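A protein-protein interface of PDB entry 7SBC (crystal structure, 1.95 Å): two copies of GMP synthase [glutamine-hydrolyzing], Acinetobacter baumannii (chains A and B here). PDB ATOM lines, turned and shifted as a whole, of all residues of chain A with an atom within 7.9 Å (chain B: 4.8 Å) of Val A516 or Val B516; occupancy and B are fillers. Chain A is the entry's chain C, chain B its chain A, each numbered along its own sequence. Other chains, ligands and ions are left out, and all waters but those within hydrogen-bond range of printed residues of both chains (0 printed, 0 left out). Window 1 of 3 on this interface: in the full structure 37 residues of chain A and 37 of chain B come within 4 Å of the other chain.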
ATOM      1  N   PHE A 436      31.304 -18.814  -0.714  1.00  0.00           N
ATOM      2  CA  PHE A 436      31.880 -17.644  -1.375  1.00  0.00           C
ATOM      3  C   PHE A 436      32.850 -18.061  -2.479  1.00  0.00           C
ATOM      4  O   PHE A 436      32.784 -17.553  -3.608  1.00  0.00           O
ATOM      5  CB  PHE A 436      32.574 -16.766  -0.331  1.00  0.00           C
ATOM      6  CG  PHE A 436      32.934 -15.379  -0.813  1.00  0.00           C
ATOM      7  CD1 PHE A 436      32.341 -14.826  -1.945  1.00  0.00           C
ATOM      8  CD2 PHE A 436      33.857 -14.616  -0.107  1.00  0.00           C
ATOM      9  CE1 PHE A 436      32.669 -13.551  -2.371  1.00  0.00           C
ATOM     10  CE2 PHE A 436      34.195 -13.328  -0.527  1.00  0.00           C
ATOM     11  CZ  PHE A 436      33.598 -12.795  -1.664  1.00  0.00           C
ATOM     12  N   PHE A 453      37.705 -13.598   0.857  1.00  0.00           N
ATOM     13  CA  PHE A 453      37.521 -14.515   1.973  1.00  0.00           C
ATOM     14  C   PHE A 453      36.342 -14.053   2.813  1.00  0.00           C
ATOM     15  O   PHE A 453      35.949 -12.883   2.781  1.00  0.00           O
ATOM     16  CB  PHE A 453      38.776 -14.613   2.850  1.00  0.00           C
ATOM     17  CG  PHE A 453      39.277 -13.287   3.365  1.00  0.00           C
ATOM     18  CD1 PHE A 453      38.797 -12.760   4.560  1.00  0.00           C
ATOM     19  CD2 PHE A 453      40.241 -12.577   2.667  1.00  0.00           C
ATOM     20  CE1 PHE A 453      39.271 -11.552   5.048  1.00  0.00           C
ATOM     21  CE2 PHE A 453      40.720 -11.365   3.148  1.00  0.00           C
ATOM     22  CZ  PHE A 453      40.233 -10.853   4.341  1.00  0.00           C
ATOM     23  N   ALA A 454      35.792 -14.993   3.567  1.00  0.00           N
ATOM     24  CA  ALA A 454      34.759 -14.685   4.542  1.00  0.00           C
ATOM     25  C   ALA A 454      35.384 -14.444   5.911  1.00  0.00           C
ATOM     26  O   ALA A 454      36.470 -14.944   6.215  1.00  0.00           O
ATOM     27  CB  ALA A 454      33.727 -15.812   4.615  1.00  0.00           C
ATOM     28  N   VAL A 455      34.683 -13.661   6.738  1.00  0.00           N
ATOM     29  CA  VAL A 455      35.093 -13.350   8.103  1.00  0.00           C
ATOM     30  C   VAL A 455      33.944 -13.692   9.038  1.00  0.00           C
ATOM     31  O   VAL A 455      32.788 -13.367   8.751  1.00  0.00           O
ATOM     32  CB  VAL A 455      35.479 -11.859   8.257  1.00  0.00           C
ATOM     33  CG1 VAL A 455      35.602 -11.477   9.742  1.00  0.00           C
ATOM     34  CG2 VAL A 455      36.758 -11.556   7.522  1.00  0.00           C
ATOM     35  N   GLN A 457      32.124 -12.780  12.278  1.00  0.00           N
ATOM     36  CA  GLN A 457      31.936 -11.812  13.355  1.00  0.00           C
ATOM     37  C   GLN A 457      31.096 -12.439  14.448  1.00  0.00           C
ATOM     38  O   GLN A 457      30.001 -12.949  14.155  1.00  0.00           O
ATOM     39  CB  GLN A 457      31.252 -10.544  12.854  1.00  0.00           C
ATOM     40  CG  GLN A 457      31.825  -9.967  11.562  1.00  0.00           C
ATOM     41  CD  GLN A 457      31.042  -8.748  11.133  1.00  0.00           C
ATOM     42  OE1 GLN A 457      31.535  -7.621  11.201  1.00  0.00           O
ATOM     43  NE2 GLN A 457      29.794  -8.966  10.728  1.00  0.00           N
ATOM     44  N   SER A 461      22.154 -11.310  14.513  1.00  0.00           N
ATOM     45  CA  SER A 461      21.067 -10.460  14.049  1.00  0.00           C
ATOM     46  C   SER A 461      19.882 -11.348  13.714  1.00  0.00           C
ATOM     47  O   SER A 461      19.994 -12.573  13.648  1.00  0.00           O
ATOM     48  CB  SER A 461      21.481  -9.601  12.834  1.00  0.00           C
ATOM     49  OG  SER A 461      21.414 -10.333  11.621  1.00  0.00           O
ATOM     50  N   VAL A 474      26.536 -13.166  12.024  1.00  0.00           N
ATOM     51  CA  VAL A 474      26.626 -12.286  10.867  1.00  0.00           C
ATOM     52  C   VAL A 474      27.987 -12.502  10.213  1.00  0.00           C
ATOM     53  O   VAL A 474      29.029 -12.236  10.827  1.00  0.00           O
ATOM     54  CB  VAL A 474      26.446 -10.813  11.262  1.00  0.00           C
ATOM     55  CG1 VAL A 474      26.467  -9.927  10.011  1.00  0.00           C
ATOM     56  CG2 VAL A 474      25.154 -10.616  12.066  1.00  0.00           C
ATOM     57  N   ILE A 475      27.980 -12.976   8.964  1.00  0.00           N
ATOM     58  CA  ILE A 475      29.203 -13.226   8.205  1.00  0.00           C
ATOM     59  C   ILE A 475      29.547 -11.985   7.394  1.00  0.00           C
ATOM     60  O   ILE A 475      28.661 -11.358   6.796  1.00  0.00           O
ATOM     61  CB  ILE A 475      29.038 -14.453   7.285  1.00  0.00           C
ATOM     62  CG1 ILE A 475      28.978 -15.751   8.102  1.00  0.00           C
ATOM     63  CG2 ILE A 475      30.144 -14.499   6.212  1.00  0.00           C
ATOM     64  CD1 ILE A 475      30.269 -16.106   8.795  1.00  0.00           C
ATOM     65  N   ALA A 476      30.836 -11.633   7.353  1.00  0.00           N
ATOM     66  CA  ALA A 476      31.336 -10.581   6.479  1.00  0.00           C
ATOM     67  C   ALA A 476      32.121 -11.188   5.321  1.00  0.00           C
ATOM     68  O   ALA A 476      32.878 -12.150   5.507  1.00  0.00           O
ATOM     69  CB  ALA A 476      32.212  -9.592   7.255  1.00  0.00           C
ATOM     70  N   LEU A 477      31.926 -10.635   4.128  1.00  0.00           N
ATOM     71  CA  LEU A 477      32.695 -10.993   2.941  1.00  0.00           C
ATOM     72  C   LEU A 477      33.733  -9.919   2.654  1.00  0.00           C
ATOM     73  O   LEU A 477      33.437  -8.725   2.718  1.00  0.00           O
ATOM     74  CB  LEU A 477      31.791 -11.144   1.718  1.00  0.00           C
ATOM     75  CG  LEU A 477      30.580 -12.067   1.868  1.00  0.00           C
ATOM     76  CD1 LEU A 477      29.778 -12.069   0.579  1.00  0.00           C
ATOM     77  CD2 LEU A 477      31.007 -13.487   2.248  1.00  0.00           C
ATOM     78  N   ARG A 478      34.950 -10.345   2.314  1.00  0.00           N
ATOM     79  CA  ARG A 478      36.024  -9.416   1.993  1.00  0.00           C
ATOM     80  C   ARG A 478      36.597  -9.800   0.637  1.00  0.00           C
ATOM     81  O   ARG A 478      36.893 -10.973   0.395  1.00  0.00           O
ATOM     82  CB  ARG A 478      37.109  -9.427   3.083  1.00  0.00           C
ATOM     83  CG  ARG A 478      38.393  -8.661   2.758  1.00  0.00           C
ATOM     84  CD  ARG A 478      38.162  -7.257   2.300  1.00  0.00           C
ATOM     85  NE  ARG A 478      39.142  -6.295   2.792  1.00  0.00           N
ATOM     86  CZ  ARG A 478      38.964  -4.984   2.695  1.00  0.00           C
ATOM     87  NH1 ARG A 478      37.922  -4.479   2.054  1.00  0.00           N
ATOM     88  NH2 ARG A 478      39.836  -4.159   3.272  1.00  0.00           N
ATOM     89  N   VAL A 498      26.816 -10.804  -5.722  1.00  0.00           N
ATOM     90  CA  VAL A 498      26.842 -10.670  -4.270  1.00  0.00           C
ATOM     91  C   VAL A 498      25.510 -11.107  -3.672  1.00  0.00           C
ATOM     92  O   VAL A 498      25.472 -11.784  -2.641  1.00  0.00           O
ATOM     93  CB  VAL A 498      27.205  -9.226  -3.877  1.00  0.00           C
ATOM     94  CG1 VAL A 498      27.102  -9.044  -2.362  1.00  0.00           C
ATOM     95  CG2 VAL A 498      28.609  -8.889  -4.360  1.00  0.00           C
ATOM     96  N   SER A 502      25.066 -14.063  -0.794  1.00  0.00           N
ATOM     97  CA  SER A 502      24.479 -13.889   0.531  1.00  0.00           C
ATOM     98  C   SER A 502      23.230 -14.743   0.688  1.00  0.00           C
ATOM     99  O   SER A 502      23.024 -15.361   1.738  1.00  0.00           O
ATOM    100  CB  SER A 502      24.175 -12.413   0.808  1.00  0.00           C
ATOM    101  OG  SER A 502      23.194 -11.902  -0.071  1.00  0.00           O
ATOM    102  N   ILE A 505      24.405 -18.285   1.370  1.00  0.00           N
ATOM    103  CA  ILE A 505      24.946 -18.463   2.714  1.00  0.00           C
ATOM    104  C   ILE A 505      23.822 -18.507   3.746  1.00  0.00           C
ATOM    105  O   ILE A 505      23.817 -19.361   4.640  1.00  0.00           O
ATOM    106  CB  ILE A 505      25.968 -17.356   3.033  1.00  0.00           C
ATOM    107  CG1 ILE A 505      27.277 -17.602   2.271  1.00  0.00           C
ATOM    108  CG2 ILE A 505      26.218 -17.282   4.542  1.00  0.00           C
ATOM    109  CD1 ILE A 505      28.254 -16.443   2.363  1.00  0.00           C
ATOM    110  N   MET A 506      22.846 -17.602   3.641  1.00  0.00           N
ATOM    111  CA  MET A 506      21.770 -17.610   4.630  1.00  0.00           C
ATOM    112  C   MET A 506      20.889 -18.838   4.477  1.00  0.00           C
ATOM    113  O   MET A 506      20.391 -19.378   5.471  1.00  0.00           O
ATOM    114  CB  MET A 506      20.922 -16.336   4.532  1.00  0.00           C
ATOM    115  CG  MET A 506      21.679 -15.085   4.924  1.00  0.00           C
ATOM    116  SD  MET A 506      20.668 -13.603   4.781  1.00  0.00           S
ATOM    117  CE  MET A 506      20.550 -13.441   2.998  1.00  0.00           C
ATOM    118  N   VAL A 512      23.862 -18.779  10.280  1.00  0.00           N
ATOM    119  CA  VAL A 512      24.159 -17.456   9.750  1.00  0.00           C
ATOM    120  C   VAL A 512      22.844 -16.739   9.469  1.00  0.00           C
ATOM    121  O   VAL A 512      22.006 -17.235   8.705  1.00  0.00           O
ATOM    122  CB  VAL A 512      25.034 -17.525   8.491  1.00  0.00           C
ATOM    123  CG1 VAL A 512      25.230 -16.131   7.908  1.00  0.00           C
ATOM    124  CG2 VAL A 512      26.381 -18.171   8.836  1.00  0.00           C
ATOM    125  N   ARG A 514      22.798 -13.359   8.407  1.00  0.00           N
ATOM    126  CA  ARG A 514      22.968 -12.158   7.609  1.00  0.00           C
ATOM    127  C   ARG A 514      24.390 -12.120   7.076  1.00  0.00           C
ATOM    128  O   ARG A 514      25.318 -12.618   7.716  1.00  0.00           O
ATOM    129  CB  ARG A 514      22.662 -10.915   8.453  1.00  0.00           C
ATOM    130  CG  ARG A 514      22.667  -9.594   7.698  1.00  0.00           C
ATOM    131  CD  ARG A 514      22.337  -8.453   8.635  1.00  0.00           C
ATOM    132  NE  ARG A 514      21.111  -8.713   9.381  1.00  0.00           N
ATOM    133  CZ  ARG A 514      19.922  -8.216   9.072  1.00  0.00           C
ATOM    134  NH1 ARG A 514      19.761  -7.405   8.038  1.00  0.00           N
ATOM    135  NH2 ARG A 514      18.873  -8.531   9.826  1.00  0.00           N
ATOM    136  N   VAL A 515      24.545 -11.525   5.896  1.00  0.00           N
ATOM    137  CA  VAL A 515      25.838 -11.356   5.241  1.00  0.00           C
ATOM    138  C   VAL A 515      26.047  -9.873   4.950  1.00  0.00           C
ATOM    139  O   VAL A 515      25.147  -9.205   4.425  1.00  0.00           O
ATOM    140  CB  VAL A 515      25.932 -12.179   3.944  1.00  0.00           C
ATOM    141  CG1 VAL A 515      27.288 -11.932   3.245  1.00  0.00           C
ATOM    142  CG2 VAL A 515      25.752 -13.658   4.233  1.00  0.00           C
ATOM    143  N   VAL A 516      27.236  -9.369   5.289  1.00  0.00           N
ATOM    144  CA  VAL A 516      27.658  -8.011   4.979  1.00  0.00           C
ATOM    145  C   VAL A 516      28.904  -8.082   4.103  1.00  0.00           C
ATOM    146  O   VAL A 516      29.594  -9.106   4.040  1.00  0.00           O
ATOM    147  CB  VAL A 516      27.944  -7.187   6.243  1.00  0.00           C
ATOM    148  CG1 VAL A 516      26.704  -7.175   7.169  1.00  0.00           C
ATOM    149  CG2 VAL A 516      29.163  -7.752   6.976  1.00  0.00           C
ATOM    150  N   TYR A 517      29.194  -6.966   3.433  1.00  0.00           N
ATOM    151  CA  TYR A 517      30.321  -6.854   2.508  1.00  0.00           C
ATOM    152  C   TYR A 517      31.243  -5.740   2.985  1.00  0.00           C
ATOM    153  O   TYR A 517      30.801  -4.601   3.152  1.00  0.00           O
ATOM    154  CB  TYR A 517      29.817  -6.556   1.095  1.00  0.00           C
ATOM    155  CG  TYR A 517      30.889  -6.526   0.022  1.00  0.00           C
ATOM    156  CD1 TYR A 517      31.827  -7.552  -0.083  1.00  0.00           C
ATOM    157  CD2 TYR A 517      30.923  -5.507  -0.917  1.00  0.00           C
ATOM    158  CE1 TYR A 517      32.795  -7.541  -1.087  1.00  0.00           C
ATOM    159  CE2 TYR A 517      31.888  -5.488  -1.929  1.00  0.00           C
ATOM    160  CZ  TYR A 517      32.817  -6.506  -2.004  1.00  0.00           C
ATOM    161  OH  TYR A 517      33.773  -6.490  -3.001  1.00  0.00           O
ATOM    162  N   ASP A 518      32.516  -6.065   3.196  1.00  0.00           N
ATOM    163  CA  ASP A 518      33.515  -5.054   3.542  1.00  0.00           C
ATOM    164  C   ASP A 518      33.634  -4.026   2.416  1.00  0.00           C
ATOM    165  O   ASP A 518      34.007  -4.370   1.291  1.00  0.00           O
ATOM    166  CB  ASP A 518      34.857  -5.742   3.792  1.00  0.00           C
ATOM    167  CG  ASP A 518      35.903  -4.822   4.404  1.00  0.00           C
ATOM    168  OD1 ASP A 518      35.788  -3.579   4.311  1.00  0.00           O
ATOM    169  OD2 ASP A 518      36.875  -5.360   4.968  1.00  0.00           O
ATOM    170  N   VAL A 519      33.297  -2.767   2.709  1.00  0.00           N
ATOM    171  CA  VAL A 519      33.348  -1.715   1.698  1.00  0.00           C
ATOM    172  C   VAL A 519      34.409  -0.693   2.079  1.00  0.00           C
ATOM    173  O   VAL A 519      34.291   0.494   1.764  1.00  0.00           O
ATOM    174  CB  VAL A 519      31.982  -1.036   1.489  1.00  0.00           C
ATOM    175  CG1 VAL A 519      31.015  -1.971   0.745  1.00  0.00           C
ATOM    176  CG2 VAL A 519      31.388  -0.547   2.832  1.00  0.00           C
ATOM    177  N   SER A 520      35.458  -1.147   2.748  1.00  0.00           N
ATOM    178  CA  SER A 520      36.553  -0.287   3.168  1.00  0.00           C
ATOM    179  C   SER A 520      37.784  -0.605   2.327  1.00  0.00           C
ATOM    180  O   SER A 520      38.202  -1.762   2.251  1.00  0.00           O
ATOM    181  CB  SER A 520      36.841  -0.481   4.657  1.00  0.00           C
ATOM    182  OG  SER A 520      35.663  -0.229   5.427  1.00  0.00           O
ATOM    183  N   TRP A 529      41.328  -8.521   8.596  1.00  0.00           N
ATOM    184  CA  TRP A 529      40.684  -7.798   9.693  1.00  0.00           C
ATOM    185  C   TRP A 529      41.488  -7.833  10.986  1.00  0.00           C
ATOM    186  O   TRP A 529      41.266  -6.983  11.863  1.00  0.00           O
ATOM    187  CB  TRP A 529      39.289  -8.369   9.960  1.00  0.00           C
ATOM    188  CG  TRP A 529      38.228  -7.982   8.946  1.00  0.00           C
ATOM    189  CD1 TRP A 529      38.381  -7.873   7.590  1.00  0.00           C
ATOM    190  CD2 TRP A 529      36.847  -7.666   9.220  1.00  0.00           C
ATOM    191  NE1 TRP A 529      37.182  -7.506   7.005  1.00  0.00           N
ATOM    192  CE2 TRP A 529      36.228  -7.375   7.985  1.00  0.00           C
ATOM    193  CE3 TRP A 529      36.080  -7.600  10.393  1.00  0.00           C
ATOM    194  CZ2 TRP A 529      34.876  -7.020   7.886  1.00  0.00           C
ATOM    195  CZ3 TRP A 529      34.735  -7.251  10.296  1.00  0.00           C
ATOM    196  CH2 TRP A 529      34.148  -6.961   9.049  1.00  0.00           C
ATOM    197  N   GLN B 457      28.208  -2.569  15.429  1.00  0.00           N
ATOM    198  CA  GLN B 457      28.592  -3.934  15.780  1.00  0.00           C
ATOM    199  C   GLN B 457      29.688  -3.877  16.827  1.00  0.00           C
ATOM    200  O   GLN B 457      30.740  -3.270  16.559  1.00  0.00           O
ATOM    201  CB  GLN B 457      29.108  -4.698  14.560  1.00  0.00           C
ATOM    202  CG  GLN B 457      28.186  -4.747  13.341  1.00  0.00           C
ATOM    203  CD  GLN B 457      28.819  -5.564  12.216  1.00  0.00           C
ATOM    204  OE1 GLN B 457      28.268  -6.573  11.774  1.00  0.00           O
ATOM    205  NE2 GLN B 457      30.003  -5.141  11.776  1.00  0.00           N
ATOM    206  N   VAL B 474      33.674  -1.868  14.153  1.00  0.00           N
ATOM    207  CA  VAL B 474      33.247  -2.093  12.774  1.00  0.00           C
ATOM    208  C   VAL B 474      31.793  -1.658  12.627  1.00  0.00           C
ATOM    209  O   VAL B 474      30.891  -2.275  13.210  1.00  0.00           O
ATOM    210  CB  VAL B 474      33.409  -3.562  12.358  1.00  0.00           C
ATOM    211  CG1 VAL B 474      32.960  -3.751  10.900  1.00  0.00           C
ATOM    212  CG2 VAL B 474      34.852  -4.025  12.561  1.00  0.00           C
ATOM    213  N   ILE B 475      31.559  -0.621  11.815  1.00  0.00           N
ATOM    214  CA  ILE B 475      30.224  -0.087  11.556  1.00  0.00           C
ATOM    215  C   ILE B 475      29.635  -0.791  10.340  1.00  0.00           C
ATOM    216  O   ILE B 475      30.339  -1.042   9.349  1.00  0.00           O
ATOM    217  CB  ILE B 475      30.285   1.440  11.329  1.00  0.00           C
ATOM    218  CG1 ILE B 475      30.614   2.172  12.631  1.00  0.00           C
ATOM    219  CG2 ILE B 475      28.986   1.968  10.690  1.00  0.00           C
ATOM    220  CD1 ILE B 475      29.544   2.025  13.696  1.00  0.00           C
ATOM    221  N   ALA B 476      28.337  -1.084  10.393  1.00  0.00           N
ATOM    222  CA  ALA B 476      27.609  -1.612   9.244  1.00  0.00           C
ATOM    223  C   ALA B 476      26.613  -0.584   8.717  1.00  0.00           C
ATOM    224  O   ALA B 476      25.940   0.110   9.492  1.00  0.00           O
ATOM    225  CB  ALA B 476      26.877  -2.912   9.601  1.00  0.00           C
ATOM    226  N   LEU B 477      26.518  -0.503   7.394  1.00  0.00           N
ATOM    227  CA  LEU B 477      25.543   0.325   6.704  1.00  0.00           C
ATOM    228  C   LEU B 477      24.406  -0.551   6.200  1.00  0.00           C
ATOM    229  O   LEU B 477      24.651  -1.591   5.582  1.00  0.00           O
ATOM    230  CB  LEU B 477      26.186   1.051   5.522  1.00  0.00           C
ATOM    231  CG  LEU B 477      27.414   1.908   5.827  1.00  0.00           C
ATOM    232  CD1 LEU B 477      27.966   2.480   4.533  1.00  0.00           C
ATOM    233  CD2 LEU B 477      27.087   3.016   6.814  1.00  0.00           C
ATOM    234  N   ARG B 514      36.550   0.345  10.355  1.00  0.00           N
ATOM    235  CA  ARG B 514      36.121  -0.327   9.140  1.00  0.00           C
ATOM    236  C   ARG B 514      34.617  -0.164   8.994  1.00  0.00           C
ATOM    237  O   ARG B 514      33.891  -0.044   9.987  1.00  0.00           O
ATOM    238  CB  ARG B 514      36.500  -1.813   9.183  1.00  0.00           C
ATOM    239  CG  ARG B 514      36.318  -2.585   7.884  1.00  0.00           C
ATOM    240  CD  ARG B 514      36.744  -4.035   8.081  1.00  0.00           C
ATOM    241  NE  ARG B 514      38.099  -4.131   8.615  1.00  0.00           N
ATOM    242  CZ  ARG B 514      39.181  -4.339   7.881  1.00  0.00           C
ATOM    243  NH1 ARG B 514      39.103  -4.531   6.573  1.00  0.00           N
ATOM    244  NH2 ARG B 514      40.371  -4.353   8.470  1.00  0.00           N
ATOM    245  N   VAL B 515      34.159  -0.158   7.745  1.00  0.00           N
ATOM    246  CA  VAL B 515      32.742  -0.064   7.427  1.00  0.00           C
ATOM    247  C   VAL B 515      32.378  -1.225   6.512  1.00  0.00           C
ATOM    248  O   VAL B 515      33.109  -1.525   5.558  1.00  0.00           O
ATOM    249  CB  VAL B 515      32.391   1.286   6.769  1.00  0.00           C
ATOM    250  CG1 VAL B 515      30.921   1.317   6.369  1.00  0.00           C
ATOM    251  CG2 VAL B 515      32.699   2.440   7.730  1.00  0.00           C
ATOM    252  N   VAL B 516      31.266  -1.886   6.818  1.00  0.00           N
ATOM    253  CA  VAL B 516      30.723  -2.935   5.969  1.00  0.00           C
ATOM    254  C   VAL B 516      29.335  -2.516   5.509  1.00  0.00           C
ATOM    255  O   VAL B 516      28.714  -1.594   6.055  1.00  0.00           O
ATOM    256  CB  VAL B 516      30.680  -4.301   6.682  1.00  0.00           C
ATOM    257  CG1 VAL B 516      32.082  -4.675   7.182  1.00  0.00           C
ATOM    258  CG2 VAL B 516      29.681  -4.265   7.836  1.00  0.00           C
ATOM    259  N   TYR B 517      28.843  -3.210   4.489  1.00  0.00           N
ATOM    260  CA  TYR B 517      27.555  -2.906   3.878  1.00  0.00           C
ATOM    261  C   TYR B 517      26.697  -4.156   3.899  1.00  0.00           C
ATOM    262  O   TYR B 517      27.140  -5.215   3.447  1.00  0.00           O
ATOM    263  CB  TYR B 517      27.736  -2.424   2.434  1.00  0.00           C
ATOM    264  CG  TYR B 517      26.442  -2.011   1.739  1.00  0.00           C
ATOM    265  CD1 TYR B 517      25.565  -1.105   2.330  1.00  0.00           C
ATOM    266  CD2 TYR B 517      26.122  -2.498   0.486  1.00  0.00           C
ATOM    267  CE1 TYR B 517      24.390  -0.716   1.689  1.00  0.00           C
ATOM    268  CE2 TYR B 517      24.949  -2.108  -0.169  1.00  0.00           C
ATOM    269  CZ  TYR B 517      24.094  -1.222   0.437  1.00  0.00           C
ATOM    270  OH  TYR B 517      22.948  -0.846  -0.222  1.00  0.00           O
ATOM    271  N   ASP B 518      25.477  -4.032   4.422  1.00  0.00           N
ATOM    272  CA  ASP B 518      24.548  -5.159   4.475  1.00  0.00           C
ATOM    273  C   ASP B 518      24.133  -5.542   3.059  1.00  0.00           C
ATOM    274  O   ASP B 518      23.511  -4.742   2.352  1.00  0.00           O
ATOM    275  CB  ASP B 518      23.326  -4.784   5.314  1.00  0.00           C
ATOM    276  CG  ASP B 518      22.445  -5.972   5.655  1.00  0.00           C
ATOM    277  OD1 ASP B 518      22.416  -6.965   4.893  1.00  0.00           O
ATOM    278  OD2 ASP B 518      21.752  -5.898   6.697  1.00  0.00           O
ATOM    279  N   VAL B 519      24.483  -6.760   2.639  1.00  0.00           N
ATOM    280  CA  VAL B 519      24.155  -7.216   1.293  1.00  0.00           C
ATOM    281  C   VAL B 519      23.149  -8.357   1.378  1.00  0.00           C
ATOM    282  O   VAL B 519      23.155  -9.273   0.549  1.00  0.00           O
ATOM    283  CB  VAL B 519      25.416  -7.621   0.497  1.00  0.00           C
ATOM    284  CG1 VAL B 519      26.207  -6.379   0.107  1.00  0.00           C
ATOM    285  CG2 VAL B 519      26.303  -8.607   1.294  1.00  0.00           C
ATOM    286  N   TRP B 529      18.284  -5.049  12.195  1.00  0.00           N
ATOM    287  CA  TRP B 529      19.110  -6.177  12.624  1.00  0.00           C
ATOM    288  C   TRP B 529      18.598  -6.835  13.902  1.00  0.00           C
ATOM    289  O   TRP B 529      18.951  -7.990  14.175  1.00  0.00           O
ATOM    290  CB  TRP B 529      20.550  -5.707  12.823  1.00  0.00           C
ATOM    291  CG  TRP B 529      21.325  -5.477  11.540  1.00  0.00           C
ATOM    292  CD1 TRP B 529      20.868  -4.920  10.372  1.00  0.00           C
ATOM    293  CD2 TRP B 529      22.700  -5.812  11.310  1.00  0.00           C
ATOM    294  NE1 TRP B 529      21.885  -4.883   9.433  1.00  0.00           N
ATOM    295  CE2 TRP B 529      23.018  -5.422   9.989  1.00  0.00           C
ATOM    296  CE3 TRP B 529      23.699  -6.396  12.100  1.00  0.00           C
ATOM    297  CZ2 TRP B 529      24.291  -5.614   9.435  1.00  0.00           C
ATOM    298  CZ3 TRP B 529      24.958  -6.582  11.552  1.00  0.00           C
ATOM    299  CH2 TRP B 529      25.245  -6.184  10.231  1.00  0.00           C
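Hydrophobic or aromatic side chains of chain A that line the printed part of chain B: Val A474, Val A498, Val A515, Val A516, Tyr A517, Val A519 and Trp A529.
Along chain B the printed residues that touch a printed residue of chain A span positions 457 to 529.
Among the printed residues, 29 pairs touch across the chains.
Among the printed residues, Asp or Glu carboxylates within 4 Å of a Lys or Arg side-chain nitrogen of the other chain: Arg A514 with Asp B518 (2.8 Å) and Asp A518 with Arg B514 (2.9 Å).
Val A515 touches Val B519, and with the chains exchanged Val A519 touches Val B515.
Val A516 touches Trp B529, and with the chains exchanged Trp A529 touches Val B516.
Tyr B517 touches its own counterpart, Tyr A517.
Tyr A517 touches Val B519, and with the chains exchanged Val A519 touches Tyr B517.
Of the 29 pairs that touch across the chains among the printed residues, 23 have their exchanged pair printed and touching as well.
Printed residues of chain B within 4 Å of Val A516: Val B516 (3.6 Å), Tyr B517 (3.2 Å), Asp B518 (3.996 Å), Val B519 (3.9 Å) and Trp B529 (3.5 Å).
Of the printed residues of chain B, Trp A529 touches Val B474 (3.9 Å), Arg B514 (3.4 Å) and Val B516 (3.6 Å).
Of the printed residues of chain A, Gln B457 touches Gln A457.
Leu B477 touches none of the printed residues of chain A.
Val B516 touches just these residues of chain A: Val A516 (3.6 Å), Tyr A517 (3.3 Å), Asp A518 (3.9 Å), Val A519 (3.9 Å) and Trp A529 (3.6 Å).
Printed residues of chain A within 4 Å of Val B519: Val A498, Ser A502, Val A515, Val A516 and Tyr A517.
The nearest printed residue of chain A that does not touch Val B516 is Ser A520 (4.9 Å).
OG of Ser A502 sits at hydrogen-bond distance from O of Val B519 (2.7 Å).
NE2 of Gln B457 lies within hydrogen-bond range of OE1 of Gln A457, at 3.0 Å.
The guanidinium group (NH1) of Arg B514 is in salt-bridge range of the side-chain carboxylate (OD2) of Asp A518 (2.9 Å).
OG of Ser A520 sits at hydrogen-bond distance from N of Val B515, at 2.8 Å.
The backbone carbonyl oxygen (O) of Val B515 lies within hydrogen-bond range of the backbone NH (N) of Val A519, at 3.1 Å.
O of Tyr B517 lies within hydrogen-bond range of N of Tyr A517 (2.7 Å).
N of Val B519 sits at hydrogen-bond distance from O of Val A515 (3.1 Å).
NH1 of Arg B514 lies close to NH2 of Arg A478.
The guanidinium group (NH1) of Arg A514 is in salt-bridge range of the side-chain carboxylate (OD2) of Asp B518, 2.8 Å away.
The backbone NH of Leu A477 sits at hydrogen-bond distance from the backbone carbonyl oxygen of Val A516, 2.8 Å away.
O of Val B474 sits close to NE2 of Gln B457 (3.3 Å).
NE of Arg A514 lies within hydrogen-bond range of OG of Ser A461, at 2.8 Å.
OD2 of Asp A518 lies within hydrogen-bond range of NE1 of Trp A529 (3.0 Å).
O of Ile B475 lies within hydrogen-bond range of N of Val B516 (2.8 Å).
The backbone carbonyl oxygen of Leu B477 sits at hydrogen-bond distance from the backbone NH of Asp B518, at 2.8 Å.
Arg A514 touches Trp B529 (CD to CE2, 3.4 Å).
Asp B518 touches Val A515 (OD1 to O, 3.6 Å).
Val A516 touches Val B516 (CG2 to CG2, 3.6 Å).
CA of Asp B518 touches CG1 of Val A516 (3.996 Å).
CG1 of Val A516 touches CH2 of Trp B529, at 3.5 Å.
O of Tyr A517 touches CA of Val B516, at 3.3 Å.
CB of Tyr A517 touches CG1 of Val B519, 3.7 Å away.
Asp A518 touches Val B515 (OD1 to O, 3.6 Å).
Asp A518 touches Val B516.
Trp A529 touches Val B516 (CH2 to CG1, 3.6 Å).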
